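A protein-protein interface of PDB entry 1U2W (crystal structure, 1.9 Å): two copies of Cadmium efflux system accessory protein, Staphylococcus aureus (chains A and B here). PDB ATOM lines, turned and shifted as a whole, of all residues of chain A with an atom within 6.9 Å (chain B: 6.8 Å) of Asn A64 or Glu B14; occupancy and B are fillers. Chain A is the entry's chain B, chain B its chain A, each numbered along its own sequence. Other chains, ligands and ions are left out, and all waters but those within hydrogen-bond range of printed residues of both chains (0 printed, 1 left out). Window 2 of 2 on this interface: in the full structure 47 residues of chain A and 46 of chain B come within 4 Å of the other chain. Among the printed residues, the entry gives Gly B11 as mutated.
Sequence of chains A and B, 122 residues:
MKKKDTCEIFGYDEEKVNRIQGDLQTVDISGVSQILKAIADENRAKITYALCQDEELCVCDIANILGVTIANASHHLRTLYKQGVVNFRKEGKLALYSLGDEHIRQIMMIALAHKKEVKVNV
Asn A64 touches four residues of chain B. Glu B14 touches just one residue of chain A: Asn A64. Of the printed residues of chain A, Lys B16 touches Asp A61. Printed residues of chain B within 4 Å of Asp A61: Tyr B12, Asp B13 and Lys B16. The nearest residue of chain B that does not touch Asn A64 is Asp B13 (5.3 Å). The nearest printed residue of chain A that does not touch Gln B21 is Leu A66 (5.0 Å).
No position is printed for both chains.
The side-chain carboxylate of Asp B13 lies close to the side-chain carboxylate of Asp A61 (2.6 Å). The side-chain amide nitrogen of Gln B21 is in hydrogen-bond range of the backbone carbonyl oxygen of Asn A64, 3.1 Å away. The side-chain carboxylate (OD2) of Asp A61 lies within salt-bridge range of the side-chain amino group (NZ) of Lys B16 (3.1 Å). O of Tyr B12 is in hydrogen-bond range of ND2 of Asn A64, at 3.1 Å. ND2 of Asn A64 sits at hydrogen-bond distance from OE1 of Glu B14 (2.9 Å). The side-chain amide nitrogen (NE2) of Gln B21 is in hydrogen-bond range of the backbone carbonyl oxygen (O) of Ile A65.
Cys A60 touches Tyr B12. Asp A61 touches Tyr B12. Val B17 touches Asn A64. Val B17 touches Ile A65.
Printed residues of chain B that touch a printed residue of chain A: Tyr B12, Asp B13, Glu B14, Lys B16, Val B17 and Gln B21. Hydrophobic or aromatic side chains of chain B that line the printed part of chain A: Tyr B12 and Val B17. Of the 13 printed residues of chain A, 4 touch a printed residue of chain B. Hydrophobic or aromatic side chains of chain A that line the printed part of chain B: Ile A65. Along chain A the printed residues that touch a printed residue of chain B span positions 60 to 65. Among the printed residues, Asp or Glu carboxylates within 4 Å of a Lys or Arg side-chain nitrogen of the other chain: Asp A61 with Lys B16 (3.1 Å).
The side-chain carboxylate (OD2) of Asp B13 lies within salt-bridge range of the side-chain amino group (NZ) of Lys B16, at 3.9 Å. ND2 of Asn B18 sits at hydrogen-bond distance from O of Glu B14, at 2.8 Å. OE1 of Glu B14 sits at hydrogen-bond distance from N of Tyr B12 (3.0 Å).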
ATOM      1  N   VAL A  59      11.975 -11.654  12.312  1.00  0.00           N
ATOM      2  CA  VAL A  59      13.398 -11.832  12.137  1.00  0.00           C
ATOM      3  C   VAL A  59      13.736 -12.460  10.764  1.00  0.00           C
ATOM      4  O   VAL A  59      14.766 -12.154  10.199  1.00  0.00           O
ATOM      5  CB  VAL A  59      14.038 -12.611  13.348  1.00  0.00           C
ATOM      6  CG1 VAL A  59      13.317 -13.959  13.603  1.00  0.00           C
ATOM      7  CG2 VAL A  59      15.544 -12.857  13.126  1.00  0.00           C
ATOM      8  N   CYS A  60      12.852 -13.325  10.267  1.00  0.00           N
ATOM      9  CA  CYS A  60      13.004 -14.019   8.992  1.00  0.00           C
ATOM     10  C   CYS A  60      12.952 -13.041   7.818  1.00  0.00           C
ATOM     11  O   CYS A  60      13.807 -13.099   6.937  1.00  0.00           O
ATOM     12  CB  CYS A  60      11.954 -15.116   8.854  1.00  0.00           C
ATOM     13  SG  CYS A  60      12.244 -16.442  10.072  1.00  0.00           S
ATOM     14  N   ASP A  61      12.013 -12.096   7.859  1.00  0.00           N
ATOM     15  CA  ASP A  61      11.952 -11.066   6.830  1.00  0.00           C
ATOM     16  C   ASP A  61      13.268 -10.288   6.836  1.00  0.00           C
ATOM     17  O   ASP A  61      13.798  -9.966   5.792  1.00  0.00           O
ATOM     18  CB  ASP A  61      10.872 -10.016   7.125  1.00  0.00           C
ATOM     19  CG  ASP A  61       9.430 -10.479   6.869  1.00  0.00           C
ATOM     20  OD1 ASP A  61       9.193 -11.423   6.091  1.00  0.00           O
ATOM     21  OD2 ASP A  61       8.521  -9.824   7.490  1.00  0.00           O
ATOM     22  N   ILE A  62      13.744  -9.942   8.029  1.00  0.00           N
ATOM     23  CA  ILE A  62      14.936  -9.076   8.162  1.00  0.00           C
ATOM     24  C   ILE A  62      16.145  -9.786   7.625  1.00  0.00           C
ATOM     25  O   ILE A  62      16.959  -9.233   6.904  1.00  0.00           O
ATOM     26  CB  ILE A  62      15.105  -8.617   9.626  1.00  0.00           C
ATOM     27  CG1 ILE A  62      14.036  -7.533   9.876  1.00  0.00           C
ATOM     28  CG2 ILE A  62      16.497  -8.084   9.864  1.00  0.00           C
ATOM     29  CD1 ILE A  62      13.585  -7.365  11.304  1.00  0.00           C
ATOM     30  N   ALA A  63      16.269 -11.050   7.978  1.00  0.00           N
ATOM     31  CA  ALA A  63      17.396 -11.823   7.491  1.00  0.00           C
ATOM     32  C   ALA A  63      17.374 -11.895   5.935  1.00  0.00           C
ATOM     33  O   ALA A  63      18.402 -11.740   5.245  1.00  0.00           O
ATOM     34  CB  ALA A  63      17.336 -13.203   8.109  1.00  0.00           C
ATOM     35  N   ASN A  64      16.198 -12.141   5.390  1.00  0.00           N
ATOM     36  CA  ASN A  64      16.061 -12.324   3.943  1.00  0.00           C
ATOM     37  C   ASN A  64      16.300 -10.951   3.228  1.00  0.00           C
ATOM     38  O   ASN A  64      16.995 -10.856   2.197  1.00  0.00           O
ATOM     39  CB  ASN A  64      14.651 -12.912   3.662  1.00  0.00           C
ATOM     40  CG  ASN A  64      14.535 -13.618   2.318  1.00  0.00           C
ATOM     41  OD1 ASN A  64      15.522 -13.835   1.616  1.00  0.00           O
ATOM     42  ND2 ASN A  64      13.306 -14.006   1.965  1.00  0.00           N
ATOM     43  N   ILE A  65      15.776  -9.885   3.797  1.00  0.00           N
ATOM     44  CA  ILE A  65      16.095  -8.555   3.255  1.00  0.00           C
ATOM     45  C   ILE A  65      17.594  -8.265   3.259  1.00  0.00           C
ATOM     46  O   ILE A  65      18.083  -7.868   2.237  1.00  0.00           O
ATOM     47  CB  ILE A  65      15.321  -7.431   3.960  1.00  0.00           C
ATOM     48  CG1 ILE A  65      13.835  -7.555   3.688  1.00  0.00           C
ATOM     49  CG2 ILE A  65      15.787  -6.031   3.526  1.00  0.00           C
ATOM     50  CD1 ILE A  65      13.040  -6.783   4.764  1.00  0.00           C
ATOM     51  N   LEU A  66      18.318  -8.493   4.379  1.00  0.00           N
ATOM     52  CA  LEU A  66      19.806  -8.319   4.434  1.00  0.00           C
ATOM     53  C   LEU A  66      20.603  -9.326   3.633  1.00  0.00           C
ATOM     54  O   LEU A  66      21.754  -9.053   3.213  1.00  0.00           O
ATOM     55  CB  LEU A  66      20.304  -8.396   5.892  1.00  0.00           C
ATOM     56  CG  LEU A  66      19.780  -7.318   6.830  1.00  0.00           C
ATOM     57  CD1 LEU A  66      20.306  -7.491   8.258  1.00  0.00           C
ATOM     58  CD2 LEU A  66      20.103  -5.953   6.291  1.00  0.00           C
ATOM     59  N   GLY A  67      20.028 -10.516   3.489  1.00  0.00           N
ATOM     60  CA  GLY A  67      20.730 -11.669   2.902  1.00  0.00           C
ATOM     61  C   GLY A  67      21.715 -12.215   3.912  1.00  0.00           C
ATOM     62  O   GLY A  67      22.866 -12.507   3.584  1.00  0.00           O
ATOM     63  N   VAL A  68      21.273 -12.325   5.158  1.00  0.00           N
ATOM     64  CA  VAL A  68      22.108 -12.882   6.207  1.00  0.00           C
ATOM     65  C   VAL A  68      21.379 -14.060   6.852  1.00  0.00           C
ATOM     66  O   VAL A  68      20.217 -14.312   6.590  1.00  0.00           O
ATOM     67  CB  VAL A  68      22.523 -11.799   7.267  1.00  0.00           C
ATOM     68  CG1 VAL A  68      23.232 -10.578   6.585  1.00  0.00           C
ATOM     69  CG2 VAL A  68      21.303 -11.299   8.027  1.00  0.00           C
ATOM     70  N   THR A  69      22.076 -14.803   7.695  1.00  0.00           N
ATOM     71  CA  THR A  69      21.414 -15.870   8.431  1.00  0.00           C
ATOM     72  C   THR A  69      20.415 -15.302   9.460  1.00  0.00           C
ATOM     73  O   THR A  69      20.535 -14.169   9.866  1.00  0.00           O
ATOM     74  CB  THR A  69      22.411 -16.767   9.151  1.00  0.00           C
ATOM     75  OG1 THR A  69      23.188 -15.998  10.090  1.00  0.00           O
ATOM     76  CG2 THR A  69      23.324 -17.527   8.154  1.00  0.00           C
ATOM     77  N   ILE A  70      19.430 -16.114   9.847  1.00  0.00           N
ATOM     78  CA  ILE A  70      18.514 -15.769  10.939  1.00  0.00           C
ATOM     79  C   ILE A  70      19.262 -15.494  12.265  1.00  0.00           C
ATOM     80  O   ILE A  70      18.940 -14.536  12.953  1.00  0.00           O
ATOM     81  CB  ILE A  70      17.438 -16.877  11.083  1.00  0.00           C
ATOM     82  CG1 ILE A  70      16.510 -16.858   9.857  1.00  0.00           C
ATOM     83  CG2 ILE A  70      16.685 -16.779  12.444  1.00  0.00           C
ATOM     84  CD1 ILE A  70      15.577 -18.095   9.754  1.00  0.00           C
ATOM     85  N   ALA A  73      20.973 -11.916  11.866  1.00  0.00           N
ATOM     86  CA  ALA A  73      19.830 -10.990  11.969  1.00  0.00           C
ATOM     87  C   ALA A  73      19.394 -10.770  13.442  1.00  0.00           C
ATOM     88  O   ALA A  73      19.225  -9.615  13.924  1.00  0.00           O
ATOM     89  CB  ALA A  73      18.674 -11.572  11.148  1.00  0.00           C
ATOM     90  N   GLY B  11      10.634 -19.623  -1.332  1.00  0.00           N
ATOM     91  CA  GLY B  11      11.238 -18.700  -0.307  1.00  0.00           C
ATOM     92  C   GLY B  11      10.258 -18.280   0.766  1.00  0.00           C
ATOM     93  O   GLY B  11       9.301 -18.977   1.054  1.00  0.00           O
ATOM     94  N   TYR B  12      10.474 -17.100   1.333  1.00  0.00           N
ATOM     95  CA  TYR B  12       9.664 -16.617   2.417  1.00  0.00           C
ATOM     96  C   TYR B  12       9.319 -15.125   2.210  1.00  0.00           C
ATOM     97  O   TYR B  12      10.241 -14.291   2.156  1.00  0.00           O
ATOM     98  CB  TYR B  12      10.455 -16.799   3.719  1.00  0.00           C
ATOM     99  CG  TYR B  12       9.676 -16.303   4.891  1.00  0.00           C
ATOM    100  CD1 TYR B  12       9.967 -15.058   5.477  1.00  0.00           C
ATOM    101  CD2 TYR B  12       8.589 -17.042   5.375  1.00  0.00           C
ATOM    102  CE1 TYR B  12       9.220 -14.593   6.555  1.00  0.00           C
ATOM    103  CE2 TYR B  12       7.840 -16.575   6.423  1.00  0.00           C
ATOM    104  CZ  TYR B  12       8.166 -15.363   7.012  1.00  0.00           C
ATOM    105  OH  TYR B  12       7.395 -14.941   8.068  1.00  0.00           O
ATOM    106  N   ASP B  13       8.024 -14.795   2.105  1.00  0.00           N
ATOM    107  CA  ASP B  13       7.606 -13.389   1.906  1.00  0.00           C
ATOM    108  C   ASP B  13       8.345 -12.688   0.773  1.00  0.00           C
ATOM    109  O   ASP B  13       8.705 -11.490   0.923  1.00  0.00           O
ATOM    110  CB  ASP B  13       7.907 -12.534   3.146  1.00  0.00           C
ATOM    111  CG  ASP B  13       6.812 -12.569   4.165  1.00  0.00           C
ATOM    112  OD1 ASP B  13       5.920 -13.469   4.079  1.00  0.00           O
ATOM    113  OD2 ASP B  13       6.852 -11.691   5.067  1.00  0.00           O
ATOM    114  N   GLU B  14       8.523 -13.357  -0.360  1.00  0.00           N
ATOM    115  CA  GLU B  14       9.510 -12.868  -1.305  1.00  0.00           C
ATOM    116  C   GLU B  14       9.041 -11.524  -1.898  1.00  0.00           C
ATOM    117  O   GLU B  14       9.850 -10.761  -2.318  1.00  0.00           O
ATOM    118  CB  GLU B  14       9.795 -13.856  -2.441  1.00  0.00           C
ATOM    119  CG  GLU B  14      10.558 -15.141  -2.038  1.00  0.00           C
ATOM    120  CD  GLU B  14      11.925 -14.826  -1.428  1.00  0.00           C
ATOM    121  OE1 GLU B  14      12.327 -15.446  -0.389  1.00  0.00           O
ATOM    122  OE2 GLU B  14      12.597 -13.928  -1.989  1.00  0.00           O
ATOM    123  N   GLU B  15       7.756 -11.298  -1.992  1.00  0.00           N
ATOM    124  CA  GLU B  15       7.326 -10.048  -2.672  1.00  0.00           C
ATOM    125  C   GLU B  15       7.627  -8.868  -1.755  1.00  0.00           C
ATOM    126  O   GLU B  15       8.256  -7.880  -2.170  1.00  0.00           O
ATOM    127  CB  GLU B  15       5.860 -10.065  -3.002  1.00  0.00           C
ATOM    128  CG  GLU B  15       5.384  -8.800  -3.589  1.00  0.00           C
ATOM    129  CD  GLU B  15       3.881  -8.758  -3.582  1.00  0.00           C
ATOM    130  OE1 GLU B  15       3.395  -7.651  -3.299  1.00  0.00           O
ATOM    131  OE2 GLU B  15       3.226  -9.827  -3.867  1.00  0.00           O
ATOM    132  N   LYS B  16       7.215  -8.991  -0.490  1.00  0.00           N
ATOM    133  CA  LYS B  16       7.539  -7.924   0.447  1.00  0.00           C
ATOM    134  C   LYS B  16       9.046  -7.767   0.606  1.00  0.00           C
ATOM    135  O   LYS B  16       9.598  -6.652   0.571  1.00  0.00           O
ATOM    136  CB  LYS B  16       6.860  -8.121   1.779  1.00  0.00           C
ATOM    137  CG  LYS B  16       7.348  -7.068   2.791  1.00  0.00           C
ATOM    138  CD  LYS B  16       6.558  -7.057   4.069  1.00  0.00           C
ATOM    139  CE  LYS B  16       6.948  -8.171   4.944  1.00  0.00           C
ATOM    140  NZ  LYS B  16       6.263  -8.018   6.265  1.00  0.00           N
ATOM    141  N   VAL B  17       9.749  -8.881   0.754  1.00  0.00           N
ATOM    142  CA  VAL B  17      11.201  -8.791   0.848  1.00  0.00           C
ATOM    143  C   VAL B  17      11.888  -8.171  -0.340  1.00  0.00           C
ATOM    144  O   VAL B  17      12.800  -7.365  -0.167  1.00  0.00           O
ATOM    145  CB  VAL B  17      11.822 -10.186   1.119  1.00  0.00           C
ATOM    146  CG1 VAL B  17      13.339 -10.124   0.958  1.00  0.00           C
ATOM    147  CG2 VAL B  17      11.412 -10.570   2.522  1.00  0.00           C
ATOM    148  N   ASN B  18      11.458  -8.531  -1.533  1.00  0.00           N
ATOM    149  CA  ASN B  18      12.110  -8.016  -2.739  1.00  0.00           C
ATOM    150  C   ASN B  18      11.818  -6.537  -2.806  1.00  0.00           C
ATOM    151  O   ASN B  18      12.660  -5.741  -3.252  1.00  0.00           O
ATOM    152  CB  ASN B  18      11.567  -8.708  -3.990  1.00  0.00           C
ATOM    153  CG  ASN B  18      11.943 -10.203  -4.065  1.00  0.00           C
ATOM    154  OD1 ASN B  18      12.949 -10.659  -3.501  1.00  0.00           O
ATOM    155  ND2 ASN B  18      11.116 -10.969  -4.761  1.00  0.00           N
ATOM    156  N   ARG B  19      10.604  -6.165  -2.410  1.00  0.00           N
ATOM    157  CA  ARG B  19      10.250  -4.727  -2.459  1.00  0.00           C
ATOM    158  C   ARG B  19      11.065  -3.835  -1.464  1.00  0.00           C
ATOM    159  O   ARG B  19      11.607  -2.767  -1.844  1.00  0.00           O
ATOM    160  CB  ARG B  19       8.698  -4.586  -2.335  1.00  0.00           C
ATOM    161  CG  ARG B  19       8.072  -3.100  -2.053  1.00  0.00           C
ATOM    162  CD  ARG B  19       6.519  -3.338  -1.644  1.00  0.00           C
ATOM    163  NE  ARG B  19       6.433  -3.097  -0.190  1.00  0.00           N
ATOM    164  CZ  ARG B  19       5.843  -3.835   0.688  1.00  0.00           C
ATOM    165  NH1 ARG B  19       5.223  -4.946   0.398  1.00  0.00           N
ATOM    166  NH2 ARG B  19       5.897  -3.400   1.925  1.00  0.00           N
ATOM    167  N   GLN B  21      14.098  -4.674  -0.268  1.00  0.00           N
ATOM    168  CA  GLN B  21      15.451  -4.629  -0.847  1.00  0.00           C
ATOM    169  C   GLN B  21      15.551  -3.544  -1.921  1.00  0.00           C
ATOM    170  O   GLN B  21      16.562  -2.844  -2.006  1.00  0.00           O
ATOM    171  CB  GLN B  21      15.760  -5.976  -1.493  1.00  0.00           C
ATOM    172  CG  GLN B  21      16.006  -7.006  -0.442  1.00  0.00           C
ATOM    173  CD  GLN B  21      16.200  -8.374  -1.024  1.00  0.00           C
ATOM    174  OE1 GLN B  21      15.604  -8.719  -2.053  1.00  0.00           O
ATOM    175  NE2 GLN B  21      17.072  -9.161  -0.391  1.00  0.00           N
